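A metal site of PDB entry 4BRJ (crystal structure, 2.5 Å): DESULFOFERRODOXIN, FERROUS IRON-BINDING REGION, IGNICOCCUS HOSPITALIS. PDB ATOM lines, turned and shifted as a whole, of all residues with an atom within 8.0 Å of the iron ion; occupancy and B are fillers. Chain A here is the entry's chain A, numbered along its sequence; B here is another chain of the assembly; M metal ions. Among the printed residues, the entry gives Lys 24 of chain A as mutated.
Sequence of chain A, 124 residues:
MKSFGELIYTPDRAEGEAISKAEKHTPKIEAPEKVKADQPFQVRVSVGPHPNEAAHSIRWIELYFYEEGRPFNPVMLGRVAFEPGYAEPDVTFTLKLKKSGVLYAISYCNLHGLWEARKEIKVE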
ATOM      1  N   ILE A  19       2.722 -34.347 -27.368  1.00  0.00           N
ATOM      2  CA  ILE A  19       2.369 -32.924 -27.411  1.00  0.00           C
ATOM      3  C   ILE A  19       3.600 -32.009 -27.306  1.00  0.00           C
ATOM      4  O   ILE A  19       3.503 -30.803 -27.506  1.00  0.00           O
ATOM      5  CB  ILE A  19       1.356 -32.522 -26.308  1.00  0.00           C
ATOM      6  CG1 ILE A  19       0.572 -31.250 -26.700  1.00  0.00           C
ATOM      7  CG2 ILE A  19       2.070 -32.332 -24.969  1.00  0.00           C
ATOM      8  CD1 ILE A  19      -0.374 -31.412 -27.894  1.00  0.00           C
ATOM      9  N   GLU A  23       4.430 -28.091 -28.721  1.00  0.00           N
ATOM     10  CA  GLU A  23       4.411 -27.058 -27.684  1.00  0.00           C
ATOM     11  C   GLU A  23       5.033 -27.540 -26.370  1.00  0.00           C
ATOM     12  O   GLU A  23       4.696 -28.614 -25.864  1.00  0.00           O
ATOM     13  CB  GLU A  23       2.969 -26.581 -27.438  1.00  0.00           C
ATOM     14  CG  GLU A  23       1.978 -27.724 -27.240  1.00  0.00           C
ATOM     15  CD  GLU A  23       0.557 -27.337 -27.594  1.00  0.00           C
ATOM     16  OE1 GLU A  23       0.226 -27.320 -28.809  1.00  0.00           O
ATOM     17  OE2 GLU A  23      -0.236 -27.062 -26.662  1.00  0.00           O
ATOM     18  N   LYS A  24       5.935 -26.744 -25.834  1.00  0.00           N
ATOM     19  CA  LYS A  24       6.585 -27.074 -24.562  1.00  0.00           C
ATOM     20  C   LYS A  24       5.793 -26.489 -23.397  1.00  0.00           C
ATOM     21  O   LYS A  24       5.433 -25.312 -23.393  1.00  0.00           O
ATOM     22  CB  LYS A  24       8.027 -26.565 -24.542  1.00  0.00           C
ATOM     23  CG  LYS A  24       8.777 -26.848 -25.827  1.00  0.00           C
ATOM     24  CD  LYS A  24       8.688 -28.321 -26.207  1.00  0.00           C
ATOM     25  CE  LYS A  24       8.961 -28.509 -27.694  1.00  0.00           C
ATOM     26  NZ  LYS A  24       8.068 -27.647 -28.519  1.00  0.00           N
ATOM     27  N   HIS A  25       5.491 -27.342 -22.420  1.00  0.00           N
ATOM     28  CA  HIS A  25       4.715 -26.910 -21.268  1.00  0.00           C
ATOM     29  C   HIS A  25       5.613 -26.794 -20.046  1.00  0.00           C
ATOM     30  O   HIS A  25       5.256 -26.148 -19.068  1.00  0.00           O
ATOM     31  CB  HIS A  25       3.586 -27.899 -20.954  1.00  0.00           C
ATOM     32  CG  HIS A  25       2.489 -27.915 -21.963  1.00  0.00           C
ATOM     33  ND1 HIS A  25       2.519 -28.723 -23.082  1.00  0.00           N
ATOM     34  CD2 HIS A  25       1.310 -27.265 -22.005  1.00  0.00           C
ATOM     35  CE1 HIS A  25       1.413 -28.554 -23.775  1.00  0.00           C
ATOM     36  NE2 HIS A  25       0.655 -27.669 -23.153  1.00  0.00           N
ATOM     37  N   VAL A  47       6.939 -20.204 -19.971  1.00  0.00           N
ATOM     38  CA  VAL A  47       6.561 -21.392 -20.704  1.00  0.00           C
ATOM     39  C   VAL A  47       6.400 -21.019 -22.169  1.00  0.00           C
ATOM     40  O   VAL A  47       5.835 -19.984 -22.486  1.00  0.00           O
ATOM     41  CB  VAL A  47       5.222 -21.955 -20.207  1.00  0.00           C
ATOM     42  CG1 VAL A  47       4.857 -23.219 -20.986  1.00  0.00           C
ATOM     43  CG2 VAL A  47       5.281 -22.251 -18.700  1.00  0.00           C
ATOM     44  N   PRO A  49       7.404 -22.478 -26.671  1.00  0.00           N
ATOM     45  CA  PRO A  49       6.255 -21.812 -27.293  1.00  0.00           C
ATOM     46  C   PRO A  49       4.976 -22.617 -27.086  1.00  0.00           C
ATOM     47  O   PRO A  49       4.935 -23.840 -27.270  1.00  0.00           O
ATOM     48  CB  PRO A  49       6.626 -21.785 -28.765  1.00  0.00           C
ATOM     49  CG  PRO A  49       7.409 -23.052 -28.954  1.00  0.00           C
ATOM     50  CD  PRO A  49       8.148 -23.307 -27.648  1.00  0.00           C
ATOM     51  N   HIS A  50       3.928 -21.905 -26.688  1.00  0.00           N
ATOM     52  CA  HIS A  50       2.637 -22.492 -26.417  1.00  0.00           C
ATOM     53  C   HIS A  50       1.597 -21.516 -26.933  1.00  0.00           C
ATOM     54  O   HIS A  50       1.854 -20.307 -26.941  1.00  0.00           O
ATOM     55  CB  HIS A  50       2.459 -22.716 -24.910  1.00  0.00           C
ATOM     56  CG  HIS A  50       1.261 -23.553 -24.564  1.00  0.00           C
ATOM     57  ND1 HIS A  50       0.079 -23.010 -24.110  1.00  0.00           N
ATOM     58  CD2 HIS A  50       1.067 -24.886 -24.647  1.00  0.00           C
ATOM     59  CE1 HIS A  50      -0.788 -23.986 -23.914  1.00  0.00           C
ATOM     60  NE2 HIS A  50      -0.219 -25.132 -24.230  1.00  0.00           N
ATOM     61  N   PRO A  51       0.431 -22.013 -27.373  1.00  0.00           N
ATOM     62  CA  PRO A  51      -0.641 -21.090 -27.781  1.00  0.00           C
ATOM     63  C   PRO A  51      -1.083 -20.235 -26.598  1.00  0.00           C
ATOM     64  O   PRO A  51      -0.813 -20.572 -25.450  1.00  0.00           O
ATOM     65  CB  PRO A  51      -1.782 -22.024 -28.198  1.00  0.00           C
ATOM     66  CG  PRO A  51      -1.104 -23.309 -28.549  1.00  0.00           C
ATOM     67  CD  PRO A  51       0.053 -23.422 -27.615  1.00  0.00           C
ATOM     68  N   ALA A  55      -9.387 -20.603 -25.634  1.00  0.00           N
ATOM     69  CA  ALA A  55      -9.600 -22.050 -25.717  1.00  0.00           C
ATOM     70  C   ALA A  55      -8.380 -22.863 -25.295  1.00  0.00           C
ATOM     71  O   ALA A  55      -8.466 -24.075 -25.105  1.00  0.00           O
ATOM     72  CB  ALA A  55     -10.028 -22.438 -27.131  1.00  0.00           C
ATOM     73  N   HIS A  56      -7.229 -22.201 -25.153  1.00  0.00           N
ATOM     74  CA  HIS A  56      -5.984 -22.908 -24.927  1.00  0.00           C
ATOM     75  C   HIS A  56      -4.832 -21.995 -24.533  1.00  0.00           C
ATOM     76  O   HIS A  56      -4.255 -21.312 -25.379  1.00  0.00           O
ATOM     77  CB  HIS A  56      -5.602 -23.694 -26.193  1.00  0.00           C
ATOM     78  CG  HIS A  56      -4.498 -24.677 -25.981  1.00  0.00           C
ATOM     79  ND1 HIS A  56      -4.026 -25.498 -26.992  1.00  0.00           N
ATOM     80  CD2 HIS A  56      -3.762 -24.985 -24.886  1.00  0.00           C
ATOM     81  CE1 HIS A  56      -3.048 -26.249 -26.537  1.00  0.00           C
ATOM     82  NE2 HIS A  56      -2.880 -25.979 -25.254  1.00  0.00           N
ATOM     83  N   SER A  57      -4.505 -21.985 -23.250  1.00  0.00           N
ATOM     84  CA  SER A  57      -3.353 -21.218 -22.773  1.00  0.00           C
ATOM     85  C   SER A  57      -2.759 -21.831 -21.495  1.00  0.00           C
ATOM     86  O   SER A  57      -3.369 -22.703 -20.856  1.00  0.00           O
ATOM     87  CB  SER A  57      -3.763 -19.759 -22.497  1.00  0.00           C
ATOM     88  OG  SER A  57      -4.640 -19.690 -21.387  1.00  0.00           O
ATOM     89  N   ILE A  58      -1.563 -21.373 -21.131  1.00  0.00           N
ATOM     90  CA  ILE A  58      -1.107 -21.550 -19.762  1.00  0.00           C
ATOM     91  C   ILE A  58      -1.896 -20.613 -18.848  1.00  0.00           C
ATOM     92  O   ILE A  58      -1.668 -19.410 -18.873  1.00  0.00           O
ATOM     93  CB  ILE A  58       0.409 -21.260 -19.599  1.00  0.00           C
ATOM     94  CG1 ILE A  58       1.233 -22.009 -20.658  1.00  0.00           C
ATOM     95  CG2 ILE A  58       0.870 -21.639 -18.217  1.00  0.00           C
ATOM     96  CD1 ILE A  58       0.933 -23.526 -20.766  1.00  0.00           C
ATOM     97  N   TYR A 108       0.098 -24.637 -15.464  1.00  0.00           N
ATOM     98  CA  TYR A 108      -1.165 -25.308 -15.749  1.00  0.00           C
ATOM     99  C   TYR A 108      -1.706 -24.899 -17.119  1.00  0.00           C
ATOM    100  O   TYR A 108      -1.819 -23.723 -17.433  1.00  0.00           O
ATOM    101  CB  TYR A 108      -2.203 -25.084 -14.647  1.00  0.00           C
ATOM    102  CG  TYR A 108      -3.540 -25.739 -14.948  1.00  0.00           C
ATOM    103  CD1 TYR A 108      -3.673 -27.129 -14.908  1.00  0.00           C
ATOM    104  CD2 TYR A 108      -4.658 -24.976 -15.307  1.00  0.00           C
ATOM    105  CE1 TYR A 108      -4.881 -27.754 -15.208  1.00  0.00           C
ATOM    106  CE2 TYR A 108      -5.884 -25.585 -15.605  1.00  0.00           C
ATOM    107  CZ  TYR A 108      -5.984 -26.988 -15.559  1.00  0.00           C
ATOM    108  OH  TYR A 108      -7.164 -27.648 -15.837  1.00  0.00           O
ATOM    109  N   CYS A 109      -1.983 -25.912 -17.946  1.00  0.00           N
ATOM    110  CA  CYS A 109      -2.625 -25.743 -19.236  1.00  0.00           C
ATOM    111  C   CYS A 109      -4.038 -26.290 -19.106  1.00  0.00           C
ATOM    112  O   CYS A 109      -4.232 -27.359 -18.545  1.00  0.00           O
ATOM    113  CB  CYS A 109      -1.857 -26.486 -20.330  1.00  0.00           C
ATOM    114  SG  CYS A 109      -2.719 -26.551 -21.933  1.00  0.00           S
ATOM    115  N   ASN A 110      -5.019 -25.564 -19.642  1.00  0.00           N
ATOM    116  CA  ASN A 110      -6.392 -25.995 -19.491  1.00  0.00           C
ATOM    117  C   ASN A 110      -6.687 -27.274 -20.267  1.00  0.00           C
ATOM    118  O   ASN A 110      -7.667 -27.962 -19.996  1.00  0.00           O
ATOM    119  CB  ASN A 110      -7.354 -24.872 -19.900  1.00  0.00           C
ATOM    120  CG  ASN A 110      -7.373 -24.651 -21.394  1.00  0.00           C
ATOM    121  OD1 ASN A 110      -6.447 -24.068 -21.956  1.00  0.00           O
ATOM    122  ND2 ASN A 110      -8.422 -25.128 -22.050  1.00  0.00           N
ATOM    123  N   LEU A 111      -5.845 -27.598 -21.244  1.00  0.00           N
ATOM    124  CA  LEU A 111      -6.025 -28.872 -21.975  1.00  0.00           C
ATOM    125  C   LEU A 111      -5.013 -29.928 -21.547  1.00  0.00           C
ATOM    126  O   LEU A 111      -5.313 -31.127 -21.517  1.00  0.00           O
ATOM    127  CB  LEU A 111      -5.911 -28.676 -23.492  1.00  0.00           C
ATOM    128  CG  LEU A 111      -6.878 -27.733 -24.192  1.00  0.00           C
ATOM    129  CD1 LEU A 111      -6.648 -27.793 -25.694  1.00  0.00           C
ATOM    130  CD2 LEU A 111      -8.321 -28.077 -23.847  1.00  0.00           C
ATOM    131  N   HIS A 112      -3.815 -29.466 -21.199  1.00  0.00           N
ATOM    132  CA  HIS A 112      -2.671 -30.361 -21.095  1.00  0.00           C
ATOM    133  C   HIS A 112      -2.148 -30.609 -19.655  1.00  0.00           C
ATOM    134  O   HIS A 112      -1.184 -31.348 -19.446  1.00  0.00           O
ATOM    135  CB  HIS A 112      -1.584 -29.922 -22.071  1.00  0.00           C
ATOM    136  CG  HIS A 112      -2.008 -30.033 -23.505  1.00  0.00           C
ATOM    137  ND1 HIS A 112      -1.675 -29.104 -24.467  1.00  0.00           N
ATOM    138  CD2 HIS A 112      -2.783 -30.963 -24.133  1.00  0.00           C
ATOM    139  CE1 HIS A 112      -2.201 -29.455 -25.621  1.00  0.00           C
ATOM    140  NE2 HIS A 112      -2.876 -30.582 -25.448  1.00  0.00           N
ATOM    141  N   GLY A 113      -2.823 -30.021 -18.670  1.00  0.00           N
ATOM    142  CA  GLY A 113      -2.566 -30.336 -17.274  1.00  0.00           C
ATOM    143  C   GLY A 113      -1.364 -29.669 -16.639  1.00  0.00           C
ATOM    144  O   GLY A 113      -1.008 -28.547 -17.008  1.00  0.00           O
ATOM    145  N   TRP A 115       2.551 -29.221 -15.344  1.00  0.00           N
ATOM    146  CA  TRP A 115       3.941 -29.472 -15.729  1.00  0.00           C
ATOM    147  C   TRP A 115       4.951 -28.845 -14.752  1.00  0.00           C
ATOM    148  O   TRP A 115       4.756 -27.713 -14.271  1.00  0.00           O
ATOM    149  CB  TRP A 115       4.187 -29.031 -17.181  1.00  0.00           C
ATOM    150  CG  TRP A 115       3.308 -29.788 -18.163  1.00  0.00           C
ATOM    151  CD1 TRP A 115       1.948 -29.726 -18.257  1.00  0.00           C
ATOM    152  CD2 TRP A 115       3.730 -30.728 -19.168  1.00  0.00           C
ATOM    153  NE1 TRP A 115       1.495 -30.556 -19.249  1.00  0.00           N
ATOM    154  CE2 TRP A 115       2.576 -31.187 -19.825  1.00  0.00           C
ATOM    155  CE3 TRP A 115       4.975 -31.213 -19.585  1.00  0.00           C
ATOM    156  CZ2 TRP A 115       2.615 -32.101 -20.878  1.00  0.00           C
ATOM    157  CZ3 TRP A 115       5.012 -32.132 -20.621  1.00  0.00           C
ATOM    158  CH2 TRP A 115       3.848 -32.570 -21.255  1.00  0.00           C
ATOM    159  N   PHE B  72      -5.478 -35.782 -21.588  1.00  0.00           N
ATOM    160  CA  PHE B  72      -4.589 -35.292 -20.545  1.00  0.00           C
ATOM    161  C   PHE B  72      -5.388 -35.069 -19.272  1.00  0.00           C
ATOM    162  O   PHE B  72      -6.607 -34.978 -19.316  1.00  0.00           O
ATOM    163  CB  PHE B  72      -3.885 -34.027 -21.001  1.00  0.00           C
ATOM    164  CG  PHE B  72      -2.983 -34.229 -22.190  1.00  0.00           C
ATOM    165  CD1 PHE B  72      -3.502 -34.350 -23.480  1.00  0.00           C
ATOM    166  CD2 PHE B  72      -1.603 -34.317 -22.029  1.00  0.00           C
ATOM    167  CE1 PHE B  72      -2.686 -34.529 -24.575  1.00  0.00           C
ATOM    168  CE2 PHE B  72      -0.769 -34.513 -23.127  1.00  0.00           C
ATOM    169  CZ  PHE B  72      -1.323 -34.625 -24.406  1.00  0.00           C
HETATM  170 FE    FE M   1      -1.144 -26.940 -23.993  1.00  0.00          FE
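Along chain A the residues within 4 Å of the iron ion span positions 23 to 112.
A ring nitrogen (NE2) of His 50 lies close to the side-chain carboxylate (OE2) of Glu 23 (3.1 Å). ND1 of His 112 sits close to OE2 of Glu 23 (3.3 Å). NE1 of Trp 115 lies within hydrogen-bond range of O of His 112. NE2 of His 56 sits close to OE2 of Glu 23 (3.2 Å). N of Leu 111 sits close to SG of Cys 109, at 3.4 Å.
NE2 of His 50 is bound to the iron ion (2.0 Å). NE2 of His 25 binds the iron ion (2.1 Å). ND1 of His 112 is bound to the iron ion, 2.3 Å away. NE2 of His 56 is bound to the iron ion (2.4 Å). The iron ion is bound by SG of Cys 109 (2.6 Å). The iron ion has five donor atoms within binding distance. Slightly farther from the iron ion lies OE2 of Glu 23 (2.8 Å).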
